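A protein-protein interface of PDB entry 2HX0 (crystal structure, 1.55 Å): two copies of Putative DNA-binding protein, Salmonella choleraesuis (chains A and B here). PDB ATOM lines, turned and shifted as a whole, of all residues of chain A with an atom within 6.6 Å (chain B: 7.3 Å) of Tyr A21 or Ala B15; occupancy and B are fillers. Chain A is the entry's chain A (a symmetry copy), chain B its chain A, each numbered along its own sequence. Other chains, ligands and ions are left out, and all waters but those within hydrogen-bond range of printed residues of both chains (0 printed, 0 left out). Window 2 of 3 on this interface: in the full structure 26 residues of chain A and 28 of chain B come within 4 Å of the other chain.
The backbone carbonyl oxygen of Ser B16 is in hydrogen-bond range of the backbone NH of Phe A20 (2.8 Å). The backbone carbonyl oxygen of Phe A20 sits close to the backbone carbonyl oxygen of Asn B14 (2.9 Å). The backbone carbonyl oxygen (O) of Asn B14 is in hydrogen-bond range of the backbone NH (N) of Ala A22, at 2.9 Å.
The guanidinium group of Arg A19 is in hydrogen-bond range of the side-chain hydroxyl of Tyr A21 (2.7 Å). ND2 of Asn B14 sits at hydrogen-bond distance from NE2 of His B12 (2.7 Å). The backbone carbonyl oxygen (O) of Arg A19 lies within hydrogen-bond range of the backbone NH (N) of Glu A124 (2.8 Å). The side-chain hydroxyl (OG) of Ser B16 is in hydrogen-bond range of the backbone NH (N) of Ala B127. The backbone carbonyl oxygen (O) of Tyr A21 lies within hydrogen-bond range of the backbone NH (N) of Ile A122.
Among the printed residues, merely in contact across the chains: Arg A19 with Ser B16, Phe A20 with Ala B15, Phe A20 with Leu B125, Tyr A21 with Asn B14, Tyr A21 with Ala B15 and Ala A22 with Phe B130.
Of the printed residues of chain B, Phe A20 touches Asn B14, Ala B15, Ser B16 and Leu B125. Of chain B, only Asn B14 and Ala B15 come within 4 Å of Tyr A21. Leu A120 touches none of the printed residues of chain B. Printed residues of chain A within 4 Å of Asn B14: Phe A20, Tyr A21 and Ala A22. Pro B126 touches none of the printed residues of chain A.
Hydrophobic or aromatic side chains of chain B within 4 Å of the printed part of chain A: Ala B15, Leu B125 and Phe B130. Of the 13 printed residues of chain A, 4 touch a printed residue of chain B. Hydrophobic or aromatic side chains of chain A within 4 Å of the printed part of chain B: Phe A20, Tyr A21 and Ala A22. Along chain A the printed residues that touch a printed residue of chain B span positions 19 to 22. Among the printed residues, 9 pairs touch across the chains. Among the printed residues, no Asp or Glu carboxylate lies within 4 Å of a Lys or Arg side-chain nitrogen of the other chain.
No position is printed for both chains. Of the 9 pairs that touch across the chains among the printed residues, none has its exchanged pair printed and touching as well.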
ATOM      1  N   ARG A  19     -29.594  21.759 -11.986  1.00  0.00           N
ATOM      2  CA  ARG A  19     -28.259  21.714 -11.416  1.00  0.00           C
ATOM      3  C   ARG A  19     -27.608  22.947 -12.034  1.00  0.00           C
ATOM      4  O   ARG A  19     -27.740  23.169 -13.234  1.00  0.00           O
ATOM      5  CB  ARG A  19     -27.530  20.441 -11.857  1.00  0.00           C
ATOM      6  CG  ARG A  19     -26.184  20.235 -11.181  1.00  0.00           C
ATOM      7  CD  ARG A  19     -25.602  18.861 -11.493  1.00  0.00           C
ATOM      8  NE  ARG A  19     -25.280  18.700 -12.907  1.00  0.00           N
ATOM      9  CZ  ARG A  19     -25.898  17.858 -13.730  1.00  0.00           C
ATOM     10  NH1 ARG A  19     -26.883  17.091 -13.286  1.00  0.00           N
ATOM     11  NH2 ARG A  19     -25.520  17.776 -14.997  1.00  0.00           N
ATOM     12  N   PHE A  20     -26.926  23.753 -11.227  1.00  0.00           N
ATOM     13  CA  PHE A  20     -26.297  24.958 -11.758  1.00  0.00           C
ATOM     14  C   PHE A  20     -24.786  24.911 -11.767  1.00  0.00           C
ATOM     15  O   PHE A  20     -24.156  24.262 -10.934  1.00  0.00           O
ATOM     16  CB  PHE A  20     -26.756  26.188 -10.979  1.00  0.00           C
ATOM     17  CG  PHE A  20     -28.217  26.468 -11.129  1.00  0.00           C
ATOM     18  CD1 PHE A  20     -29.149  25.863 -10.286  1.00  0.00           C
ATOM     19  CD2 PHE A  20     -28.673  27.289 -12.153  1.00  0.00           C
ATOM     20  CE1 PHE A  20     -30.521  26.074 -10.467  1.00  0.00           C
ATOM     21  CE2 PHE A  20     -30.039  27.506 -12.343  1.00  0.00           C
ATOM     22  CZ  PHE A  20     -30.960  26.896 -11.498  1.00  0.00           C
ATOM     23  N   TYR A  21     -24.216  25.619 -12.731  1.00  0.00           N
ATOM     24  CA  TYR A  21     -22.773  25.697 -12.892  1.00  0.00           C
ATOM     25  C   TYR A  21     -22.361  27.155 -12.943  1.00  0.00           C
ATOM     26  O   TYR A  21     -23.001  27.963 -13.609  1.00  0.00           O
ATOM     27  CB  TYR A  21     -22.335  25.029 -14.192  1.00  0.00           C
ATOM     28  CG  TYR A  21     -22.598  23.546 -14.268  1.00  0.00           C
ATOM     29  CD1 TYR A  21     -23.839  23.058 -14.658  1.00  0.00           C
ATOM     30  CD2 TYR A  21     -21.595  22.629 -13.962  1.00  0.00           C
ATOM     31  CE1 TYR A  21     -24.077  21.686 -14.747  1.00  0.00           C
ATOM     32  CE2 TYR A  21     -21.822  21.257 -14.048  1.00  0.00           C
ATOM     33  CZ  TYR A  21     -23.062  20.794 -14.441  1.00  0.00           C
ATOM     34  OH  TYR A  21     -23.273  19.438 -14.534  1.00  0.00           O
ATOM     35  N   ALA A  22     -21.288  27.492 -12.241  1.00  0.00           N
ATOM     36  CA  ALA A  22     -20.802  28.861 -12.258  1.00  0.00           C
ATOM     37  C   ALA A  22     -19.432  28.863 -12.915  1.00  0.00           C
ATOM     38  O   ALA A  22     -18.588  28.027 -12.601  1.00  0.00           O
ATOM     39  CB  ALA A  22     -20.703  29.413 -10.833  1.00  0.00           C
ATOM     40  N   LEU A  23     -19.210  29.782 -13.842  1.00  0.00           N
ATOM     41  CA  LEU A  23     -17.908  29.839 -14.485  1.00  0.00           C
ATOM     42  C   LEU A  23     -17.557  31.240 -14.927  1.00  0.00           C
ATOM     43  O   LEU A  23     -18.423  32.100 -15.060  1.00  0.00           O
ATOM     44  CB  LEU A  23     -17.850  28.893 -15.683  1.00  0.00           C
ATOM     45  CG  LEU A  23     -18.855  29.096 -16.818  1.00  0.00           C
ATOM     46  CD1 LEU A  23     -18.259  28.587 -18.128  1.00  0.00           C
ATOM     47  CD2 LEU A  23     -20.155  28.372 -16.492  1.00  0.00           C
ATOM     48  N   PHE A  38     -17.808  23.890 -22.551  1.00  0.00           N
ATOM     49  CA  PHE A  38     -18.360  23.610 -21.230  1.00  0.00           C
ATOM     50  C   PHE A  38     -19.492  22.591 -21.342  1.00  0.00           C
ATOM     51  O   PHE A  38     -19.633  21.699 -20.501  1.00  0.00           O
ATOM     52  CB  PHE A  38     -18.883  24.896 -20.598  1.00  0.00           C
ATOM     53  CG  PHE A  38     -19.116  24.791 -19.119  1.00  0.00           C
ATOM     54  CD1 PHE A  38     -18.050  24.886 -18.230  1.00  0.00           C
ATOM     55  CD2 PHE A  38     -20.395  24.578 -18.614  1.00  0.00           C
ATOM     56  CE1 PHE A  38     -18.249  24.773 -16.851  1.00  0.00           C
ATOM     57  CE2 PHE A  38     -20.612  24.462 -17.233  1.00  0.00           C
ATOM     58  CZ  PHE A  38     -19.536  24.560 -16.349  1.00  0.00           C
ATOM     59  N   ASN A  42     -19.250  18.754 -19.606  1.00  0.00           N
ATOM     60  CA  ASN A  42     -20.228  18.271 -18.644  1.00  0.00           C
ATOM     61  C   ASN A  42     -21.386  17.499 -19.262  1.00  0.00           C
ATOM     62  O   ASN A  42     -22.329  17.127 -18.562  1.00  0.00           O
ATOM     63  CB  ASN A  42     -20.762  19.451 -17.830  1.00  0.00           C
ATOM     64  CG  ASN A  42     -19.673  20.144 -17.041  1.00  0.00           C
ATOM     65  OD1 ASN A  42     -19.170  21.197 -17.435  1.00  0.00           O
ATOM     66  ND2 ASN A  42     -19.289  19.544 -15.926  1.00  0.00           N
ATOM     67  N   LEU A  44     -23.890  18.347 -21.033  1.00  0.00           N
ATOM     68  CA  LEU A  44     -25.180  18.965 -20.747  1.00  0.00           C
ATOM     69  C   LEU A  44     -26.159  18.677 -21.886  1.00  0.00           C
ATOM     70  O   LEU A  44     -25.836  18.879 -23.058  1.00  0.00           O
ATOM     71  CB  LEU A  44     -25.001  20.474 -20.559  1.00  0.00           C
ATOM     72  CG  LEU A  44     -23.991  20.877 -19.477  1.00  0.00           C
ATOM     73  CD1 LEU A  44     -23.985  22.396 -19.322  1.00  0.00           C
ATOM     74  CD2 LEU A  44     -24.339  20.199 -18.156  1.00  0.00           C
ATOM     75  N   LEU A 120     -20.791  33.589 -15.799  1.00  0.00           N
ATOM     76  CA  LEU A 120     -21.990  32.867 -16.183  1.00  0.00           C
ATOM     77  C   LEU A 120     -22.499  31.881 -15.153  1.00  0.00           C
ATOM     78  O   LEU A 120     -21.722  31.235 -14.458  1.00  0.00           O
ATOM     79  CB  LEU A 120     -21.722  32.066 -17.461  1.00  0.00           C
ATOM     80  CG  LEU A 120     -21.412  32.757 -18.784  1.00  0.00           C
ATOM     81  CD1 LEU A 120     -20.403  31.930 -19.563  1.00  0.00           C
ATOM     82  CD2 LEU A 120     -22.701  32.927 -19.576  1.00  0.00           C
ATOM     83  N   VAL A 121     -23.820  31.784 -15.056  1.00  0.00           N
ATOM     84  CA  VAL A 121     -24.446  30.782 -14.208  1.00  0.00           C
ATOM     85  C   VAL A 121     -25.300  30.026 -15.217  1.00  0.00           C
ATOM     86  O   VAL A 121     -26.212  30.594 -15.824  1.00  0.00           O
ATOM     87  CB  VAL A 121     -25.340  31.373 -13.115  1.00  0.00           C
ATOM     88  CG1 VAL A 121     -26.056  30.235 -12.382  1.00  0.00           C
ATOM     89  CG2 VAL A 121     -24.500  32.150 -12.134  1.00  0.00           C
ATOM     90  N   ILE A 122     -24.970  28.759 -15.429  1.00  0.00           N
ATOM     91  CA  ILE A 122     -25.691  27.939 -16.387  1.00  0.00           C
ATOM     92  C   ILE A 122     -26.521  26.875 -15.687  1.00  0.00           C
ATOM     93  O   ILE A 122     -26.026  26.170 -14.815  1.00  0.00           O
ATOM     94  CB  ILE A 122     -24.704  27.255 -17.357  1.00  0.00           C
ATOM     95  CG1 ILE A 122     -23.950  28.328 -18.156  1.00  0.00           C
ATOM     96  CG2 ILE A 122     -25.452  26.295 -18.279  1.00  0.00           C
ATOM     97  CD1 ILE A 122     -22.998  29.183 -17.389  1.00  0.00           C
ATOM     98  N   GLY A 123     -27.791  26.777 -16.065  1.00  0.00           N
ATOM     99  CA  GLY A 123     -28.655  25.773 -15.472  1.00  0.00           C
ATOM    100  C   GLY A 123     -28.782  24.577 -16.397  1.00  0.00           C
ATOM    101  O   GLY A 123     -28.769  24.731 -17.615  1.00  0.00           O
ATOM    102  N   GLU A 124     -28.871  23.386 -15.813  1.00  0.00           N
ATOM    103  CA  GLU A 124     -29.033  22.139 -16.565  1.00  0.00           C
ATOM    104  C   GLU A 124     -30.256  21.444 -15.966  1.00  0.00           C
ATOM    105  O   GLU A 124     -30.414  21.403 -14.746  1.00  0.00           O
ATOM    106  CB  GLU A 124     -27.795  21.244 -16.413  1.00  0.00           C
ATOM    107  CG  GLU A 124     -28.022  19.764 -16.772  1.00  0.00           C
ATOM    108  CD  GLU A 124     -28.097  19.487 -18.270  1.00  0.00           C
ATOM    109  OE1 GLU A 124     -28.323  20.428 -19.056  1.00  0.00           O
ATOM    110  OE2 GLU A 124     -27.937  18.312 -18.666  1.00  0.00           O
ATOM    111  N   HIS B  12     -13.955  20.834  -6.176  1.00  0.00           N
ATOM    112  CA  HIS B  12     -14.100  21.486  -7.510  1.00  0.00           C
ATOM    113  C   HIS B  12     -15.268  22.465  -7.487  1.00  0.00           C
ATOM    114  O   HIS B  12     -16.179  22.340  -6.668  1.00  0.00           O
ATOM    115  CB  HIS B  12     -14.325  20.425  -8.593  1.00  0.00           C
ATOM    116  CG  HIS B  12     -14.401  20.983  -9.981  1.00  0.00           C
ATOM    117  ND1 HIS B  12     -13.422  21.795 -10.512  1.00  0.00           N
ATOM    118  CD2 HIS B  12     -15.331  20.832 -10.953  1.00  0.00           C
ATOM    119  CE1 HIS B  12     -13.746  22.120 -11.751  1.00  0.00           C
ATOM    120  NE2 HIS B  12     -14.900  21.547 -12.043  1.00  0.00           N
ATOM    121  N   HIS B  13     -15.243  23.440  -8.387  1.00  0.00           N
ATOM    122  CA  HIS B  13     -16.301  24.433  -8.426  1.00  0.00           C
ATOM    123  C   HIS B  13     -17.426  24.140  -9.407  1.00  0.00           C
ATOM    124  O   HIS B  13     -17.759  22.989  -9.677  1.00  0.00           O
ATOM    125  CB  HIS B  13     -15.714  25.814  -8.723  1.00  0.00           C
ATOM    126  CG  HIS B  13     -14.698  25.817  -9.821  1.00  0.00           C
ATOM    127  ND1 HIS B  13     -13.445  25.262  -9.672  1.00  0.00           N
ATOM    128  CD2 HIS B  13     -14.755  26.286 -11.090  1.00  0.00           C
ATOM    129  CE1 HIS B  13     -12.773  25.389 -10.802  1.00  0.00           C
ATOM    130  NE2 HIS B  13     -13.545  26.006 -11.679  1.00  0.00           N
ATOM    131  N   ASN B  14     -17.992  25.226  -9.921  1.00  0.00           N
ATOM    132  CA  ASN B  14     -19.100  25.250 -10.866  1.00  0.00           C
ATOM    133  C   ASN B  14     -20.410  24.569 -10.492  1.00  0.00           C
ATOM    134  O   ASN B  14     -21.445  25.225 -10.512  1.00  0.00           O
ATOM    135  CB  ASN B  14     -18.651  24.788 -12.273  1.00  0.00           C
ATOM    136  CG  ASN B  14     -17.953  23.439 -12.275  1.00  0.00           C
ATOM    137  OD1 ASN B  14     -18.530  22.418 -11.904  1.00  0.00           O
ATOM    138  ND2 ASN B  14     -16.701  23.432 -12.716  1.00  0.00           N
ATOM    139  N   ALA B  15     -20.391  23.294 -10.112  1.00  0.00           N
ATOM    140  CA  ALA B  15     -21.655  22.598  -9.821  1.00  0.00           C
ATOM    141  C   ALA B  15     -22.306  22.770  -8.447  1.00  0.00           C
ATOM    142  O   ALA B  15     -21.656  22.626  -7.411  1.00  0.00           O
ATOM    143  CB  ALA B  15     -21.493  21.118 -10.118  1.00  0.00           C
ATOM    144  N   SER B  16     -23.609  23.050  -8.454  1.00  0.00           N
ATOM    145  CA  SER B  16     -24.356  23.217  -7.212  1.00  0.00           C
ATOM    146  C   SER B  16     -25.863  23.280  -7.420  1.00  0.00           C
ATOM    147  O   SER B  16     -26.340  23.672  -8.486  1.00  0.00           O
ATOM    148  CB  SER B  16     -23.913  24.501  -6.499  1.00  0.00           C
ATOM    149  OG  SER B  16     -24.628  24.696  -5.289  1.00  0.00           O
ATOM    150  N   THR B  17     -26.610  22.876  -6.396  1.00  0.00           N
ATOM    151  CA  THR B  17     -28.060  22.976  -6.437  1.00  0.00           C
ATOM    152  C   THR B  17     -28.251  24.448  -6.080  1.00  0.00           C
ATOM    153  O   THR B  17     -27.289  25.125  -5.713  1.00  0.00           O
ATOM    154  CB  THR B  17     -28.717  22.124  -5.340  1.00  0.00           C
ATOM    155  OG1 THR B  17     -28.225  22.541  -4.060  1.00  0.00           O
ATOM    156  CG2 THR B  17     -28.394  20.653  -5.546  1.00  0.00           C
ATOM    157  N   LEU B 125     -26.040  29.472  -4.464  1.00  0.00           N
ATOM    158  CA  LEU B 125     -25.467  28.154  -4.751  1.00  0.00           C
ATOM    159  C   LEU B 125     -24.751  27.668  -3.489  1.00  0.00           C
ATOM    160  O   LEU B 125     -23.575  27.961  -3.281  1.00  0.00           O
ATOM    161  CB  LEU B 125     -24.486  28.280  -5.921  1.00  0.00           C
ATOM    162  CG  LEU B 125     -25.126  28.889  -7.175  1.00  0.00           C
ATOM    163  CD1 LEU B 125     -24.051  29.377  -8.137  1.00  0.00           C
ATOM    164  CD2 LEU B 125     -26.029  27.857  -7.829  1.00  0.00           C
ATOM    165  N   PRO B 126     -25.454  26.892  -2.641  1.00  0.00           N
ATOM    166  CA  PRO B 126     -24.901  26.376  -1.386  1.00  0.00           C
ATOM    167  C   PRO B 126     -23.602  25.577  -1.430  1.00  0.00           C
ATOM    168  O   PRO B 126     -22.893  25.515  -0.428  1.00  0.00           O
ATOM    169  CB  PRO B 126     -26.058  25.558  -0.805  1.00  0.00           C
ATOM    170  CG  PRO B 126     -27.282  26.198  -1.406  1.00  0.00           C
ATOM    171  CD  PRO B 126     -26.832  26.407  -2.833  1.00  0.00           C
ATOM    172  N   ALA B 127     -23.280  24.968  -2.566  1.00  0.00           N
ATOM    173  CA  ALA B 127     -22.055  24.178  -2.654  1.00  0.00           C
ATOM    174  C   ALA B 127     -20.842  24.990  -3.094  1.00  0.00           C
ATOM    175  O   ALA B 127     -19.721  24.472  -3.138  1.00  0.00           O
ATOM    176  CB  ALA B 127     -22.264  22.997  -3.606  1.00  0.00           C
ATOM    177  N   LEU B 128     -21.054  26.265  -3.401  1.00  0.00           N
ATOM    178  CA  LEU B 128     -19.964  27.114  -3.866  1.00  0.00           C
ATOM    179  C   LEU B 128     -19.800  28.396  -3.063  1.00  0.00           C
ATOM    180  O   LEU B 128     -20.663  28.772  -2.276  1.00  0.00           O
ATOM    181  CB  LEU B 128     -20.203  27.496  -5.331  1.00  0.00           C
ATOM    182  CG  LEU B 128     -20.431  26.353  -6.325  1.00  0.00           C
ATOM    183  CD1 LEU B 128     -20.896  26.928  -7.654  1.00  0.00           C
ATOM    184  CD2 LEU B 128     -19.148  25.551  -6.510  1.00  0.00           C
ATOM    185  N   PHE B 130     -18.301  32.433  -3.846  1.00  0.00           N
ATOM    186  CA  PHE B 130     -17.760  33.401  -4.793  1.00  0.00           C
ATOM    187  C   PHE B 130     -16.850  34.360  -4.041  1.00  0.00           C
ATOM    188  O   PHE B 130     -17.115  34.714  -2.889  1.00  0.00           O
ATOM    189  CB  PHE B 130     -18.859  34.255  -5.439  1.00  0.00           C
ATOM    190  CG  PHE B 130     -19.765  33.517  -6.388  1.00  0.00           C
ATOM    191  CD1 PHE B 130     -19.437  32.254  -6.875  1.00  0.00           C
ATOM    192  CD2 PHE B 130     -20.949  34.113  -6.815  1.00  0.00           C
ATOM    193  CE1 PHE B 130     -20.278  31.595  -7.777  1.00  0.00           C
ATOM    194  CE2 PHE B 130     -21.798  33.469  -7.714  1.00  0.00           C
ATOM    195  CZ  PHE B 130     -21.462  32.205  -8.197  1.00  0.00           C
ATOM    196  N   ILE B 145     -14.377  31.077  -8.154  1.00  0.00           N
ATOM    197  CA  ILE B 145     -15.354  30.121  -7.651  1.00  0.00           C
ATOM    198  C   ILE B 145     -14.676  28.939  -6.975  1.00  0.00           C
ATOM    199  O   ILE B 145     -13.843  28.269  -7.581  1.00  0.00           O
ATOM    200  CB  ILE B 145     -16.218  29.577  -8.798  1.00  0.00           C
ATOM    201  CG1 ILE B 145     -16.796  30.737  -9.606  1.00  0.00           C
ATOM    202  CG2 ILE B 145     -17.339  28.714  -8.243  1.00  0.00           C
ATOM    203  CD1 ILE B 145     -15.850  31.327 -10.642  1.00  0.00           C
